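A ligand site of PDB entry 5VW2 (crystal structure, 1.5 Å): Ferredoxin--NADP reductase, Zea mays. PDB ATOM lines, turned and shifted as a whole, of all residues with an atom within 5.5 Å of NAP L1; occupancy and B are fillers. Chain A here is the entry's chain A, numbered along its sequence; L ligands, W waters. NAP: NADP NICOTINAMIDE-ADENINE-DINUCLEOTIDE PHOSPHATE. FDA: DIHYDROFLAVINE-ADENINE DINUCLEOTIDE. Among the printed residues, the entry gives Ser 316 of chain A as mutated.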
ATOM      1  N   PRO A  50      -8.904  -1.613 -10.906  1.00  0.00           N
ATOM      2  CA  PRO A  50      -9.725  -1.735  -9.677  1.00  0.00           C
ATOM      3  C   PRO A  50     -11.187  -2.054  -9.934  1.00  0.00           C
ATOM      4  O   PRO A  50     -11.875  -2.547  -9.038  1.00  0.00           O
ATOM      5  CB  PRO A  50      -9.560  -0.374  -8.993  1.00  0.00           C
ATOM      6  CG  PRO A  50      -9.103   0.542 -10.072  1.00  0.00           C
ATOM      7  CD  PRO A  50      -8.284  -0.294 -11.009  1.00  0.00           C
ATOM      8  N   THR A  53     -14.661  -1.813 -16.555  1.00  0.00           N
ATOM      9  CA  THR A  53     -15.259  -0.847 -17.460  1.00  0.00           C
ATOM     10  C   THR A  53     -15.469  -1.595 -18.760  1.00  0.00           C
ATOM     11  O   THR A  53     -14.560  -2.263 -19.246  1.00  0.00           O
ATOM     12  CB  THR A  53     -14.342   0.352 -17.673  1.00  0.00           C
ATOM     13  OG1 THR A  53     -14.176   1.036 -16.432  1.00  0.00           O
ATOM     14  CG2 THR A  53     -14.954   1.338 -18.648  1.00  0.00           C
ATOM     15  N   SER A  71     -25.444  12.393 -24.893  1.00  0.00           N
ATOM     16  CA  SER A  71     -25.676  11.242 -24.057  1.00  0.00           C
ATOM     17  C   SER A  71     -26.918  10.495 -24.517  1.00  0.00           C
ATOM     18  O   SER A  71     -27.842  11.087 -25.058  1.00  0.00           O
ATOM     19  CB  SER A  71     -25.916  11.622 -22.587  1.00  0.00           C
ATOM     20  OG  SER A  71     -24.789  12.256 -22.020  1.00  0.00           O
ATOM     21  N   SER A  94     -22.615   8.860 -21.595  1.00  0.00           N
ATOM     22  CA  SER A  94     -21.999   9.684 -22.611  1.00  0.00           C
ATOM     23  C   SER A  94     -21.646   8.821 -23.806  1.00  0.00           C
ATOM     24  O   SER A  94     -20.987   7.783 -23.683  1.00  0.00           O
ATOM     25  CB  SER A  94     -20.740  10.302 -22.033  1.00  0.00           C
ATOM     26  OG  SER A  94     -21.089  11.205 -21.004  1.00  0.00           O
ATOM     27  N   ARG A 114     -18.580   2.173 -16.517  1.00  0.00           N
ATOM     28  CA  ARG A 114     -17.940   1.625 -15.326  1.00  0.00           C
ATOM     29  C   ARG A 114     -18.973   0.877 -14.506  1.00  0.00           C
ATOM     30  O   ARG A 114     -20.030   1.430 -14.173  1.00  0.00           O
ATOM     31  CB  ARG A 114     -17.364   2.768 -14.485  1.00  0.00           C
ATOM     32  CG  ARG A 114     -16.795   2.321 -13.141  1.00  0.00           C
ATOM     33  CD  ARG A 114     -15.544   1.480 -13.315  1.00  0.00           C
ATOM     34  NE  ARG A 114     -15.031   0.964 -12.033  1.00  0.00           N
ATOM     35  CZ  ARG A 114     -14.170   1.597 -11.244  1.00  0.00           C
ATOM     36  NH1 ARG A 114     -13.793   1.027 -10.105  1.00  0.00           N
ATOM     37  NH2 ARG A 114     -13.670   2.788 -11.576  1.00  0.00           N
ATOM     38  N   THR A 173     -11.270  11.857 -16.741  1.00  0.00           N
ATOM     39  CA  THR A 173     -10.986  10.846 -15.752  1.00  0.00           C
ATOM     40  C   THR A 173     -11.873   9.638 -16.016  1.00  0.00           C
ATOM     41  O   THR A 173     -13.088   9.773 -16.152  1.00  0.00           O
ATOM     42  CB  THR A 173     -11.191  11.352 -14.319  1.00  0.00           C
ATOM     43  OG1 THR A 173     -12.380  12.127 -14.235  1.00  0.00           O
ATOM     44  CG2 THR A 173      -9.990  12.192 -13.886  1.00  0.00           C
ATOM     45  N   GLY A 174     -11.250   8.467 -16.102  1.00  0.00           N
ATOM     46  CA  GLY A 174     -11.990   7.224 -16.264  1.00  0.00           C
ATOM     47  C   GLY A 174     -12.869   7.251 -17.491  1.00  0.00           C
ATOM     48  O   GLY A 174     -12.458   7.710 -18.571  1.00  0.00           O
ATOM     49  N   THR A 175     -14.112   6.803 -17.318  1.00  0.00           N
ATOM     50  CA  THR A 175     -15.079   6.764 -18.408  1.00  0.00           C
ATOM     51  C   THR A 175     -15.477   8.144 -18.903  1.00  0.00           C
ATOM     52  O   THR A 175     -16.150   8.243 -19.920  1.00  0.00           O
ATOM     53  CB  THR A 175     -16.336   5.982 -17.999  1.00  0.00           C
ATOM     54  OG1 THR A 175     -16.894   6.540 -16.816  1.00  0.00           O
ATOM     55  CG2 THR A 175     -15.996   4.525 -17.781  1.00  0.00           C
ATOM     56  N   GLY A 176     -15.046   9.209 -18.223  1.00  0.00           N
ATOM     57  CA  GLY A 176     -15.152  10.544 -18.783  1.00  0.00           C
ATOM     58  C   GLY A 176     -14.466  10.701 -20.123  1.00  0.00           C
ATOM     59  O   GLY A 176     -14.705  11.694 -20.815  1.00  0.00           O
ATOM     60  N   ALA A 178     -15.221   9.100 -22.608  1.00  0.00           N
ATOM     61  CA  ALA A 178     -16.230   8.765 -23.623  1.00  0.00           C
ATOM     62  C   ALA A 178     -16.415   9.787 -24.735  1.00  0.00           C
ATOM     63  O   ALA A 178     -16.247   9.445 -25.914  1.00  0.00           O
ATOM     64  CB  ALA A 178     -17.573   8.430 -22.946  1.00  0.00           C
ATOM     65  N   PRO A 179     -16.809  11.035 -24.445  1.00  0.00           N
ATOM     66  CA  PRO A 179     -17.066  11.974 -25.540  1.00  0.00           C
ATOM     67  C   PRO A 179     -15.838  12.196 -26.376  1.00  0.00           C
ATOM     68  O   PRO A 179     -15.933  12.457 -27.586  1.00  0.00           O
ATOM     69  CB  PRO A 179     -17.488  13.265 -24.836  1.00  0.00           C
ATOM     70  CG  PRO A 179     -16.888  13.142 -23.422  1.00  0.00           C
ATOM     71  CD  PRO A 179     -17.033  11.668 -23.121  1.00  0.00           C
ATOM     72  N   GLY A 206      -6.822  10.483 -17.050  1.00  0.00           N
ATOM     73  CA  GLY A 206      -6.455   9.945 -15.752  1.00  0.00           C
ATOM     74  C   GLY A 206      -7.160   8.625 -15.479  1.00  0.00           C
ATOM     75  O   GLY A 206      -8.391   8.568 -15.544  1.00  0.00           O
ATOM     76  N   VAL A 207      -6.393   7.565 -15.223  1.00  0.00           N
ATOM     77  CA  VAL A 207      -6.905   6.250 -14.849  1.00  0.00           C
ATOM     78  C   VAL A 207      -6.008   5.677 -13.774  1.00  0.00           C
ATOM     79  O   VAL A 207      -4.919   6.202 -13.504  1.00  0.00           O
ATOM     80  CB  VAL A 207      -7.001   5.288 -16.049  1.00  0.00           C
ATOM     81  CG1 VAL A 207      -7.984   5.798 -17.114  1.00  0.00           C
ATOM     82  CG2 VAL A 207      -5.628   5.025 -16.638  1.00  0.00           C
ATOM     83  N   ALA A 208      -6.489   4.632 -13.103  1.00  0.00           N
ATOM     84  CA  ALA A 208      -5.812   4.128 -11.915  1.00  0.00           C
ATOM     85  C   ALA A 208      -4.438   3.573 -12.242  1.00  0.00           C
ATOM     86  O   ALA A 208      -3.471   3.820 -11.517  1.00  0.00           O
ATOM     87  CB  ALA A 208      -6.689   3.073 -11.233  1.00  0.00           C
ATOM     88  N   ALA A 235      -2.238  10.211 -16.767  1.00  0.00           N
ATOM     89  CA  ALA A 235      -1.950  10.286 -15.345  1.00  0.00           C
ATOM     90  C   ALA A 235      -2.437   8.983 -14.731  1.00  0.00           C
ATOM     91  O   ALA A 235      -3.644   8.756 -14.639  1.00  0.00           O
ATOM     92  CB  ALA A 235      -2.674  11.475 -14.713  1.00  0.00           C
ATOM     93  N   SER A 237      -2.910   7.145 -11.586  1.00  0.00           N
ATOM     94  CA  SER A 237      -2.924   7.624 -10.202  1.00  0.00           C
ATOM     95  C   SER A 237      -2.221   6.654  -9.264  1.00  0.00           C
ATOM     96  O   SER A 237      -1.517   7.087  -8.339  1.00  0.00           O
ATOM     97  CB  SER A 237      -4.353   7.876  -9.741  1.00  0.00           C
ATOM     98  OG  SER A 237      -5.169   6.720  -9.883  1.00  0.00           O
ATOM     99  N   ARG A 238      -2.397   5.355  -9.482  1.00  0.00           N
ATOM    100  CA  ARG A 238      -1.827   4.372  -8.565  1.00  0.00           C
ATOM    101  C   ARG A 238      -0.469   3.859  -9.017  1.00  0.00           C
ATOM    102  O   ARG A 238       0.126   3.031  -8.321  1.00  0.00           O
ATOM    103  CB  ARG A 238      -2.831   3.227  -8.354  1.00  0.00           C
ATOM    104  CG  ARG A 238      -4.199   3.768  -7.968  1.00  0.00           C
ATOM    105  CD  ARG A 238      -5.219   2.728  -7.575  1.00  0.00           C
ATOM    106  NE  ARG A 238      -6.502   3.360  -7.296  1.00  0.00           N
ATOM    107  CZ  ARG A 238      -7.574   2.739  -6.799  1.00  0.00           C
ATOM    108  NH1 ARG A 238      -7.512   1.456  -6.514  1.00  0.00           N
ATOM    109  NH2 ARG A 238      -8.691   3.421  -6.600  1.00  0.00           N
ATOM    110  N   LYS A 247      -1.107  11.116  -5.158  1.00  0.00           N
ATOM    111  CA  LYS A 247      -1.320  10.333  -6.364  1.00  0.00           C
ATOM    112  C   LYS A 247      -1.358  11.258  -7.564  1.00  0.00           C
ATOM    113  O   LYS A 247      -1.869  12.386  -7.500  1.00  0.00           O
ATOM    114  CB  LYS A 247      -2.612   9.538  -6.240  1.00  0.00           C
ATOM    115  CG  LYS A 247      -2.519   8.378  -5.272  1.00  0.00           C
ATOM    116  CD  LYS A 247      -3.509   7.269  -5.611  1.00  0.00           C
ATOM    117  CE  LYS A 247      -4.897   7.576  -5.094  1.00  0.00           C
ATOM    118  NZ  LYS A 247      -5.722   6.339  -4.956  1.00  0.00           N
ATOM    119  N   TYR A 249      -2.716  12.817 -10.489  1.00  0.00           N
ATOM    120  CA  TYR A 249      -4.012  13.050 -11.102  1.00  0.00           C
ATOM    121  C   TYR A 249      -3.818  13.880 -12.359  1.00  0.00           C
ATOM    122  O   TYR A 249      -2.726  14.379 -12.672  1.00  0.00           O
ATOM    123  CB  TYR A 249      -4.937  13.736 -10.090  1.00  0.00           C
ATOM    124  CG  TYR A 249      -5.509  12.827  -9.013  1.00  0.00           C
ATOM    125  CD1 TYR A 249      -5.556  11.444  -9.158  1.00  0.00           C
ATOM    126  CD2 TYR A 249      -6.040  13.369  -7.842  1.00  0.00           C
ATOM    127  CE1 TYR A 249      -6.091  10.635  -8.170  1.00  0.00           C
ATOM    128  CE2 TYR A 249      -6.585  12.563  -6.854  1.00  0.00           C
ATOM    129  CZ  TYR A 249      -6.607  11.192  -7.024  1.00  0.00           C
ATOM    130  OH  TYR A 249      -7.151  10.390  -6.045  1.00  0.00           O
ATOM    131  N   VAL A 250      -4.903  13.988 -13.137  1.00  0.00           N
ATOM    132  CA  VAL A 250      -4.826  14.789 -14.355  1.00  0.00           C
ATOM    133  C   VAL A 250      -4.410  16.225 -14.072  1.00  0.00           C
ATOM    134  O   VAL A 250      -3.732  16.841 -14.895  1.00  0.00           O
ATOM    135  CB  VAL A 250      -6.140  14.731 -15.164  1.00  0.00           C
ATOM    136  CG1 VAL A 250      -6.330  13.390 -15.759  1.00  0.00           C
ATOM    137  CG2 VAL A 250      -7.333  15.144 -14.310  1.00  0.00           C
ATOM    138  N   GLN A 251      -4.826  16.793 -12.931  1.00  0.00           N
ATOM    139  CA  GLN A 251      -4.450  18.177 -12.649  1.00  0.00           C
ATOM    140  C   GLN A 251      -2.942  18.328 -12.560  1.00  0.00           C
ATOM    141  O   GLN A 251      -2.392  19.390 -12.898  1.00  0.00           O
ATOM    142  CB  GLN A 251      -5.107  18.696 -11.364  1.00  0.00           C
ATOM    143  CG  GLN A 251      -5.077  17.748 -10.182  1.00  0.00           C
ATOM    144  CD  GLN A 251      -6.327  16.865 -10.105  1.00  0.00           C
ATOM    145  OE1 GLN A 251      -6.811  16.393 -11.133  1.00  0.00           O
ATOM    146  NE2 GLN A 251      -6.850  16.658  -8.900  1.00  0.00           N
ATOM    147  N   CYS A 274     -14.448  16.033 -18.418  1.00  0.00           N
ATOM    148  CA  CYS A 274     -15.497  15.028 -18.326  1.00  0.00           C
ATOM    149  C   CYS A 274     -15.008  13.903 -17.434  1.00  0.00           C
ATOM    150  O   CYS A 274     -13.849  13.491 -17.495  1.00  0.00           O
ATOM    151  CB  CYS A 274     -15.848  14.508 -19.736  1.00  0.00           C
ATOM    152  SG  CYS A 274     -17.297  13.481 -19.774  1.00  0.00           S
ATOM    153  N   GLY A 275     -15.919  13.410 -16.598  1.00  0.00           N
ATOM    154  CA  GLY A 275     -15.628  12.328 -15.664  1.00  0.00           C
ATOM    155  C   GLY A 275     -16.084  12.639 -14.254  1.00  0.00           C
ATOM    156  O   GLY A 275     -17.181  13.136 -14.062  1.00  0.00           O
ATOM    157  N   LEU A 276     -15.203  12.377 -13.298  1.00  0.00           N
ATOM    158  CA  LEU A 276     -15.519  12.513 -11.888  1.00  0.00           C
ATOM    159  C   LEU A 276     -15.699  13.975 -11.500  1.00  0.00           C
ATOM    160  O   LEU A 276     -14.820  14.800 -11.760  1.00  0.00           O
ATOM    161  CB  LEU A 276     -14.343  12.005 -11.064  1.00  0.00           C
ATOM    162  CG  LEU A 276     -13.856  10.574 -11.170  1.00  0.00           C
ATOM    163  CD1 LEU A 276     -12.412  10.518 -10.713  1.00  0.00           C
ATOM    164  CD2 LEU A 276     -14.708   9.681 -10.313  1.00  0.00           C
ATOM    165  N   GLY A 278     -15.268  15.056  -8.656  1.00  0.00           N
ATOM    166  CA  GLY A 278     -14.237  15.365  -7.679  1.00  0.00           C
ATOM    167  C   GLY A 278     -12.961  15.900  -8.286  1.00  0.00           C
ATOM    168  O   GLY A 278     -12.148  16.488  -7.572  1.00  0.00           O
ATOM    169  N   MET A 279     -12.758  15.717  -9.588  1.00  0.00           N
ATOM    170  CA  MET A 279     -11.526  16.249 -10.149  1.00  0.00           C
ATOM    171  C   MET A 279     -11.558  17.766 -10.308  1.00  0.00           C
ATOM    172  O   MET A 279     -10.490  18.378 -10.394  1.00  0.00           O
ATOM    173  CB  MET A 279     -11.172  15.593 -11.475  1.00  0.00           C
ATOM    174  CG  MET A 279     -12.046  16.022 -12.608  1.00  0.00           C
ATOM    175  SD  MET A 279     -11.467  15.372 -14.160  1.00  0.00           S
ATOM    176  CE  MET A 279     -12.989  15.655 -14.986  1.00  0.00           C
ATOM    177  N   GLU A 314     -18.657  18.640 -18.044  1.00  0.00           N
ATOM    178  CA  GLU A 314     -19.749  17.696 -17.777  1.00  0.00           C
ATOM    179  C   GLU A 314     -19.173  16.607 -16.884  1.00  0.00           C
ATOM    180  O   GLU A 314     -18.450  15.713 -17.342  1.00  0.00           O
ATOM    181  CB  GLU A 314     -20.338  17.164 -19.082  1.00  0.00           C
ATOM    182  CG  GLU A 314     -21.870  17.038 -19.038  1.00  0.00           C
ATOM    183  CD  GLU A 314     -22.456  16.457 -20.307  1.00  0.00           C
ATOM    184  OE1 GLU A 314     -22.165  15.277 -20.618  1.00  0.00           O
ATOM    185  OE2 GLU A 314     -23.212  17.161 -21.001  1.00  0.00           O
ATOM    186  N   VAL A 315     -19.446  16.714 -15.584  1.00  0.00           N
ATOM    187  CA  VAL A 315     -18.885  15.796 -14.593  1.00  0.00           C
ATOM    188  C   VAL A 315     -20.007  15.426 -13.645  1.00  0.00           C
ATOM    189  O   VAL A 315     -21.013  16.118 -13.545  1.00  0.00           O
ATOM    190  CB  VAL A 315     -17.715  16.403 -13.817  1.00  0.00           C
ATOM    191  CG1 VAL A 315     -16.559  16.720 -14.747  1.00  0.00           C
ATOM    192  CG2 VAL A 315     -18.138  17.663 -13.060  1.00  0.00           C
ATOM    193  N   SER A 316     -19.823  14.308 -12.960  1.00  0.00           N
ATOM    194  CA  SER A 316     -20.830  13.874 -12.009  1.00  0.00           C
ATOM    195  C   SER A 316     -20.257  12.868 -11.035  1.00  0.00           C
ATOM    196  O   SER A 316     -19.083  12.498 -11.101  1.00  0.00           O
ATOM    197  CB  SER A 316     -22.005  13.254 -12.747  1.00  0.00           C
ATOM    198  OG  SER A 316     -21.595  12.105 -13.458  1.00  0.00           O
ATOM    199  OXT SER A 316     -20.991  12.395 -10.149  1.00  0.00           O
HETATM  200  PA  NAP L   1     -12.221   5.929 -11.491  1.00  0.00           P
HETATM  201  O1A NAP L   1     -11.328   4.740 -11.720  1.00  0.00           O
HETATM  202  O2A NAP L   1     -13.083   5.992 -10.236  1.00  0.00           O
HETATM  203  O5B NAP L   1     -11.310   7.231 -11.521  1.00  0.00           O
HETATM  204  C5B NAP L   1     -10.616   7.619 -12.707  1.00  0.00           C
HETATM  205  C4B NAP L   1      -9.325   8.265 -12.265  1.00  0.00           C
HETATM  206  O4B NAP L   1      -9.567   9.527 -11.622  1.00  0.00           O
HETATM  207  C3B NAP L   1      -8.641   7.393 -11.243  1.00  0.00           C
HETATM  208  O3B NAP L   1      -7.251   7.358 -11.529  1.00  0.00           O
HETATM  209  C2B NAP L   1      -8.837   8.073  -9.920  1.00  0.00           C
HETATM  210  O2B NAP L   1      -7.754   7.782  -9.045  1.00  0.00           O
HETATM  211  C1B NAP L   1      -8.834   9.509 -10.400  1.00  0.00           C
HETATM  212  N9A NAP L   1      -9.371  10.420  -9.392  1.00  0.00           N
HETATM  213  C8A NAP L   1     -10.073  10.127  -8.271  1.00  0.00           C
HETATM  214  N7A NAP L   1     -10.350  11.262  -7.590  1.00  0.00           N
HETATM  215  C5A NAP L   1      -9.794  12.278  -8.283  1.00  0.00           C
HETATM  216  C6A NAP L   1      -9.696  13.744  -8.135  1.00  0.00           C
HETATM  217  N6A NAP L   1     -10.269  14.350  -7.065  1.00  0.00           N
HETATM  218  N1A NAP L   1      -9.019  14.416  -9.078  1.00  0.00           N
HETATM  219  C2A NAP L   1      -8.457  13.811 -10.139  1.00  0.00           C
HETATM  220  N3A NAP L   1      -8.505  12.483 -10.340  1.00  0.00           N
HETATM  221  C4A NAP L   1      -9.146  11.704  -9.450  1.00  0.00           C
HETATM  222  O3  NAP L   1     -13.020   6.149 -12.854  1.00  0.00           O
HETATM  223  PN  NAP L   1     -14.550   5.903 -13.265  1.00  0.00           P
HETATM  224  O1N NAP L   1     -15.277   5.065 -12.257  1.00  0.00           O
HETATM  225  O2N NAP L   1     -14.514   5.606 -14.733  1.00  0.00           O
HETATM  226  O5D NAP L   1     -14.905   7.440 -13.001  1.00  0.00           O
HETATM  227  C5D NAP L   1     -15.412   8.275 -14.003  1.00  0.00           C
HETATM  228  C4D NAP L   1     -16.681   8.799 -13.397  1.00  0.00           C
HETATM  229  O4D NAP L   1     -17.193   9.826 -14.218  1.00  0.00           O
HETATM  230  C3D NAP L   1     -17.729   7.708 -13.259  1.00  0.00           C
HETATM  231  O3D NAP L   1     -18.198   7.653 -11.911  1.00  0.00           O
HETATM  232  C2D NAP L   1     -18.824   8.114 -14.213  1.00  0.00           C
HETATM  233  O2D NAP L   1     -20.114   7.834 -13.670  1.00  0.00           O
HETATM  234  C1D NAP L   1     -18.574   9.615 -14.418  1.00  0.00           C
HETATM  235  N1N NAP L   1     -18.872  10.109 -15.754  1.00  0.00           N
HETATM  236  C2N NAP L   1     -19.582  11.242 -15.872  1.00  0.00           C
HETATM  237  C3N NAP L   1     -19.866  11.746 -17.129  1.00  0.00           C
HETATM  238  C7N NAP L   1     -20.684  12.994 -17.243  1.00  0.00           C
HETATM  239  O7N NAP L   1     -21.135  13.525 -16.237  1.00  0.00           O
HETATM  240  N7N NAP L   1     -20.941  13.516 -18.427  1.00  0.00           N
HETATM  241  C4N NAP L   1     -19.406  11.064 -18.250  1.00  0.00           C
HETATM  242  C5N NAP L   1     -18.660   9.913 -18.091  1.00  0.00           C
HETATM  243  C6N NAP L   1     -18.384   9.476 -16.823  1.00  0.00           C
HETATM  244  P2B NAP L   1      -7.922   6.906  -7.694  1.00  0.00           P
HETATM  245  O1X NAP L   1      -8.101   7.960  -6.625  1.00  0.00           O
HETATM  246  O2X NAP L   1      -9.138   6.027  -7.834  1.00  0.00           O
HETATM  247  O3X NAP L   1      -6.590   6.206  -7.692  1.00  0.00           O
HETATM  248  PA  FDA L   2     -27.532   3.175  -9.257  1.00  0.00           P
HETATM  249  O1A FDA L   2     -28.171   4.445  -9.682  1.00  0.00           O
HETATM  250  O2A FDA L   2     -28.381   1.928  -9.104  1.00  0.00           O
HETATM  251  O5B FDA L   2     -26.759   3.417  -7.868  1.00  0.00           O
HETATM  252  C5B FDA L   2     -25.987   4.601  -7.700  1.00  0.00           C
HETATM  253  C4B FDA L   2     -24.833   4.300  -6.777  1.00  0.00           C
HETATM  254  O4B FDA L   2     -25.340   3.960  -5.477  1.00  0.00           O
HETATM  255  C3B FDA L   2     -24.000   3.090  -7.191  1.00  0.00           C
HETATM  256  O3B FDA L   2     -22.620   3.388  -6.983  1.00  0.00           O
HETATM  257  C2B FDA L   2     -24.433   1.974  -6.262  1.00  0.00           C
HETATM  258  O2B FDA L   2     -23.422   0.998  -6.096  1.00  0.00           O
HETATM  259  C1B FDA L   2     -24.727   2.765  -5.020  1.00  0.00           C
HETATM  260  N9A FDA L   2     -25.710   2.159  -4.114  1.00  0.00           N
HETATM  261  C8A FDA L   2     -26.890   1.617  -4.433  1.00  0.00           C
HETATM  262  N7A FDA L   2     -27.536   1.184  -3.320  1.00  0.00           N
HETATM  263  C5A FDA L   2     -26.742   1.485  -2.280  1.00  0.00           C
HETATM  264  C6A FDA L   2     -26.782   1.323  -0.819  1.00  0.00           C
HETATM  265  N6A FDA L   2     -27.864   0.734  -0.281  1.00  0.00           N
HETATM  266  N1A FDA L   2     -25.726   1.757  -0.106  1.00  0.00           N
HETATM  267  C2A FDA L   2     -24.655   2.347  -0.666  1.00  0.00           C
HETATM  268  N3A FDA L   2     -24.548   2.515  -2.000  1.00  0.00           N
HETATM  269  C4A FDA L   2     -25.542   2.105  -2.804  1.00  0.00           C
HETATM  270  N1  FDA L   2     -21.174   6.659 -16.156  1.00  0.00           N
HETATM  271  C2  FDA L   2     -20.391   5.902 -16.911  1.00  0.00           C
HETATM  272  O2  FDA L   2     -19.850   4.893 -16.400  1.00  0.00           O
HETATM  273  N3  FDA L   2     -20.152   6.206 -18.193  1.00  0.00           N
HETATM  274  C4  FDA L   2     -20.680   7.280 -18.797  1.00  0.00           C
HETATM  275  O4  FDA L   2     -20.470   7.533 -20.004  1.00  0.00           O
HETATM  276  C4X FDA L   2     -21.569   8.158 -18.025  1.00  0.00           C
HETATM  277  N5  FDA L   2     -22.092   9.275 -18.540  1.00  0.00           N
HETATM  278  C5X FDA L   2     -22.848  10.079 -17.787  1.00  0.00           C
HETATM  279  C6  FDA L   2     -23.320  11.282 -18.309  1.00  0.00           C
HETATM  280  C7  FDA L   2     -24.068  12.167 -17.538  1.00  0.00           C
HETATM  281  C7M FDA L   2     -24.566  13.475 -18.103  1.00  0.00           C
HETATM  282  C8  FDA L   2     -24.335  11.816 -16.138  1.00  0.00           C
HETATM  283  C8M FDA L   2     -25.123  12.739 -15.253  1.00  0.00           C
HETATM  284  C9  FDA L   2     -23.878  10.632 -15.622  1.00  0.00           C
HETATM  285  C9A FDA L   2     -23.132   9.741 -16.374  1.00  0.00           C
HETATM  286  N10 FDA L   2     -22.629   8.537 -15.848  1.00  0.00           N
HETATM  287  C10 FDA L   2     -21.780   7.754 -16.625  1.00  0.00           C
HETATM  288  C1' FDA L   2     -23.149   7.951 -14.602  1.00  0.00           C
HETATM  289  C2' FDA L   2     -24.350   7.051 -14.907  1.00  0.00           C
HETATM  290  O2' FDA L   2     -25.411   7.855 -15.403  1.00  0.00           O
HETATM  291  C3' FDA L   2     -24.854   6.334 -13.659  1.00  0.00           C
HETATM  292  O3' FDA L   2     -25.151   7.263 -12.626  1.00  0.00           O
HETATM  293  C4' FDA L   2     -23.868   5.292 -13.179  1.00  0.00           C
HETATM  294  O4' FDA L   2     -23.658   4.354 -14.226  1.00  0.00           O
HETATM  295  C5' FDA L   2     -24.432   4.522 -12.000  1.00  0.00           C
HETATM  296  O5' FDA L   2     -25.764   4.119 -12.333  1.00  0.00           O
HETATM  297  P   FDA L   2     -26.300   2.711 -11.814  1.00  0.00           P
HETATM  298  O1P FDA L   2     -27.716   2.577 -12.268  1.00  0.00           O
HETATM  299  O2P FDA L   2     -25.320   1.645 -12.118  1.00  0.00           O
HETATM  300  O3P FDA L   2     -26.251   2.860 -10.184  1.00  0.00           O
HETATM  301  O   HOH W   1      -5.534   9.605 -12.596  1.00  0.00           O
HETATM  302  O   HOH W   2      -6.803  11.999 -12.601  1.00  0.00           O
HETATM  303  O   HOH W   3     -10.020  17.521  -6.533  1.00  0.00           O
HETATM  304  O   HOH W   4     -12.299  12.096  -5.188  1.00  0.00           O
HETATM  305  O   HOH W   5     -13.043   3.443 -15.784  1.00  0.00           O
HETATM  306  O   HOH W   6     -20.321   4.918 -11.697  1.00  0.00           O
HETATM  307  O   HOH W   7      -9.352   4.222 -13.586  1.00  0.00           O
HETATM  308  O   HOH W   8      -9.794   4.024  -9.625  1.00  0.00           O
HETATM  309  O   HOH W   9     -22.865  15.791 -15.831  1.00  0.00           O
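The backbone carbonyl oxygen (O) of Gly 275 lies close to an oxygen (O4D) of NAP L1, at 3.3 Å. Residues that only touch NAP L1: Met 279, Gly 174, Val 315, Gly 206, Thr 173, Cys 274 and Gly 176. Hydrophobic or aromatic side chains within 4 Å of NAP L1: Tyr 249, Leu 276 and Met 279. The nearest printed residue that does not touch NAP L1 is Val 250 (4.5 Å).
The backbone NH (N) of Gly 174 sits at hydrogen-bond distance from the backbone carbonyl oxygen (O) of Gly 206 (2.9 Å). The backbone NH of Val 207 lies within hydrogen-bond range of the backbone carbonyl oxygen of Ala 235. The backbone NH (N) of Thr 173 lies within hydrogen-bond range of the backbone carbonyl oxygen (O) of Cys 274 (3.1 Å). The side-chain sulfur (SD) of Met 279 lies within hydrogen-bond range of the side-chain hydroxyl (OG1) of Thr 173, at 3.4 Å. SG of Cys 274 lies close to O of Gly 176. O of Glu 314 sits close to SG of Cys 274 (3.5 Å). N of Leu 276 sits at hydrogen-bond distance from OG1 of Thr 173, at 3.0 Å. The backbone NH (N) of Arg 238 sits at hydrogen-bond distance from the backbone carbonyl oxygen (O) of Ala 208 (2.8 Å).
A nitrogen (N1) of FDA L2 lies within hydrogen-bond range of an oxygen (O2D) of NAP L1 (2.9 Å).
An oxygen (O2N) of NAP L1 sits at hydrogen-bond distance from the backbone NH (N) of Thr 175, at 2.9 Å. N of Arg 114 lies within hydrogen-bond range of O2 of FDA L2, at 3.0 Å. The backbone NH (N) of Leu 276 is in hydrogen-bond range of an oxygen (O4D) of NAP L1. The backbone carbonyl oxygen of Gly 278 sits at hydrogen-bond distance from a nitrogen (N6A) of NAP L1. An oxygen (O1X) of NAP L1 is in hydrogen-bond range of the side-chain hydroxyl (OH) of Tyr 249 (2.7 Å). The side-chain amino group (NZ) of Lys 247 lies within salt-bridge range of an oxygen (O3X) of NAP L1, at 2.9 Å. OG of Ser 316 is in hydrogen-bond range of O7N of NAP L1, at 3.2 Å. OG of Ser 94 sits close to N7N of NAP L1 (3.5 Å). N1A of NAP L1 lies within hydrogen-bond range of NE2 of Gln 251 (3.1 Å). O1N of NAP L1 lies within salt-bridge range of NH2 of Arg 114, 2.9 Å away. The side-chain carboxylate (OE1) of Glu 314 lies within hydrogen-bond range of a nitrogen (N7N) of NAP L1, at 3.1 Å. A nitrogen (N7N) of NAP L1 is in hydrogen-bond range of the backbone carbonyl oxygen (O) of Glu 314. The backbone NH of Ser 94 lies within hydrogen-bond range of an oxygen (O4) of FDA L2 (3.0 Å). The side-chain hydroxyl (OG1) of Thr 175 is in hydrogen-bond range of an oxygen (O2) of FDA L2, 3.4 Å away. An oxygen (O3B) of NAP L1 sits at hydrogen-bond distance from the backbone NH of Ala 208 (3.2 Å). The backbone carbonyl oxygen (O) of Val 207 lies close to an oxygen (O3B) of NAP L1. NE of Arg 238 is in salt-bridge range of O3X of NAP L1, at 2.9 Å. The side-chain hydroxyl (OG) of Ser 94 is in hydrogen-bond range of a nitrogen (N5) of FDA L2. The side-chain hydroxyl (OG1) of Thr 175 sits close to an oxygen (O2N) of NAP L1. The side-chain hydroxyl (OG) of Ser 237 sits at hydrogen-bond distance from an oxygen (O3X) of NAP L1 (2.7 Å).
Water W8 lies within hydrogen-bond range of an oxygen (O1A) of NAP L1 (2.7 Å) and the guanidinium group (NH2) of Arg 238 (3.3 Å). Water W5 lies within hydrogen-bond range of the side-chain hydroxyl of Thr 53 (2.7 Å) and an oxygen (O2N) of NAP L1 (2.8 Å). Water W2 bridges N of Val 250 and N3A of NAP L1. Water W9 bridges an oxygen (O7N) of NAP L1 and the backbone carbonyl oxygen (O) of Val 315. Water W1 lies within hydrogen-bond range of the backbone carbonyl oxygen (O) of Ala 235 (2.9 Å), an oxygen (O3B) of NAP L1 (3.0 Å) and the backbone NH (N) of Val 207 (3.4 Å). Water W3 lies within hydrogen-bond range of the backbone carbonyl oxygen of Gly 278 and a nitrogen (N6A) of NAP L1.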
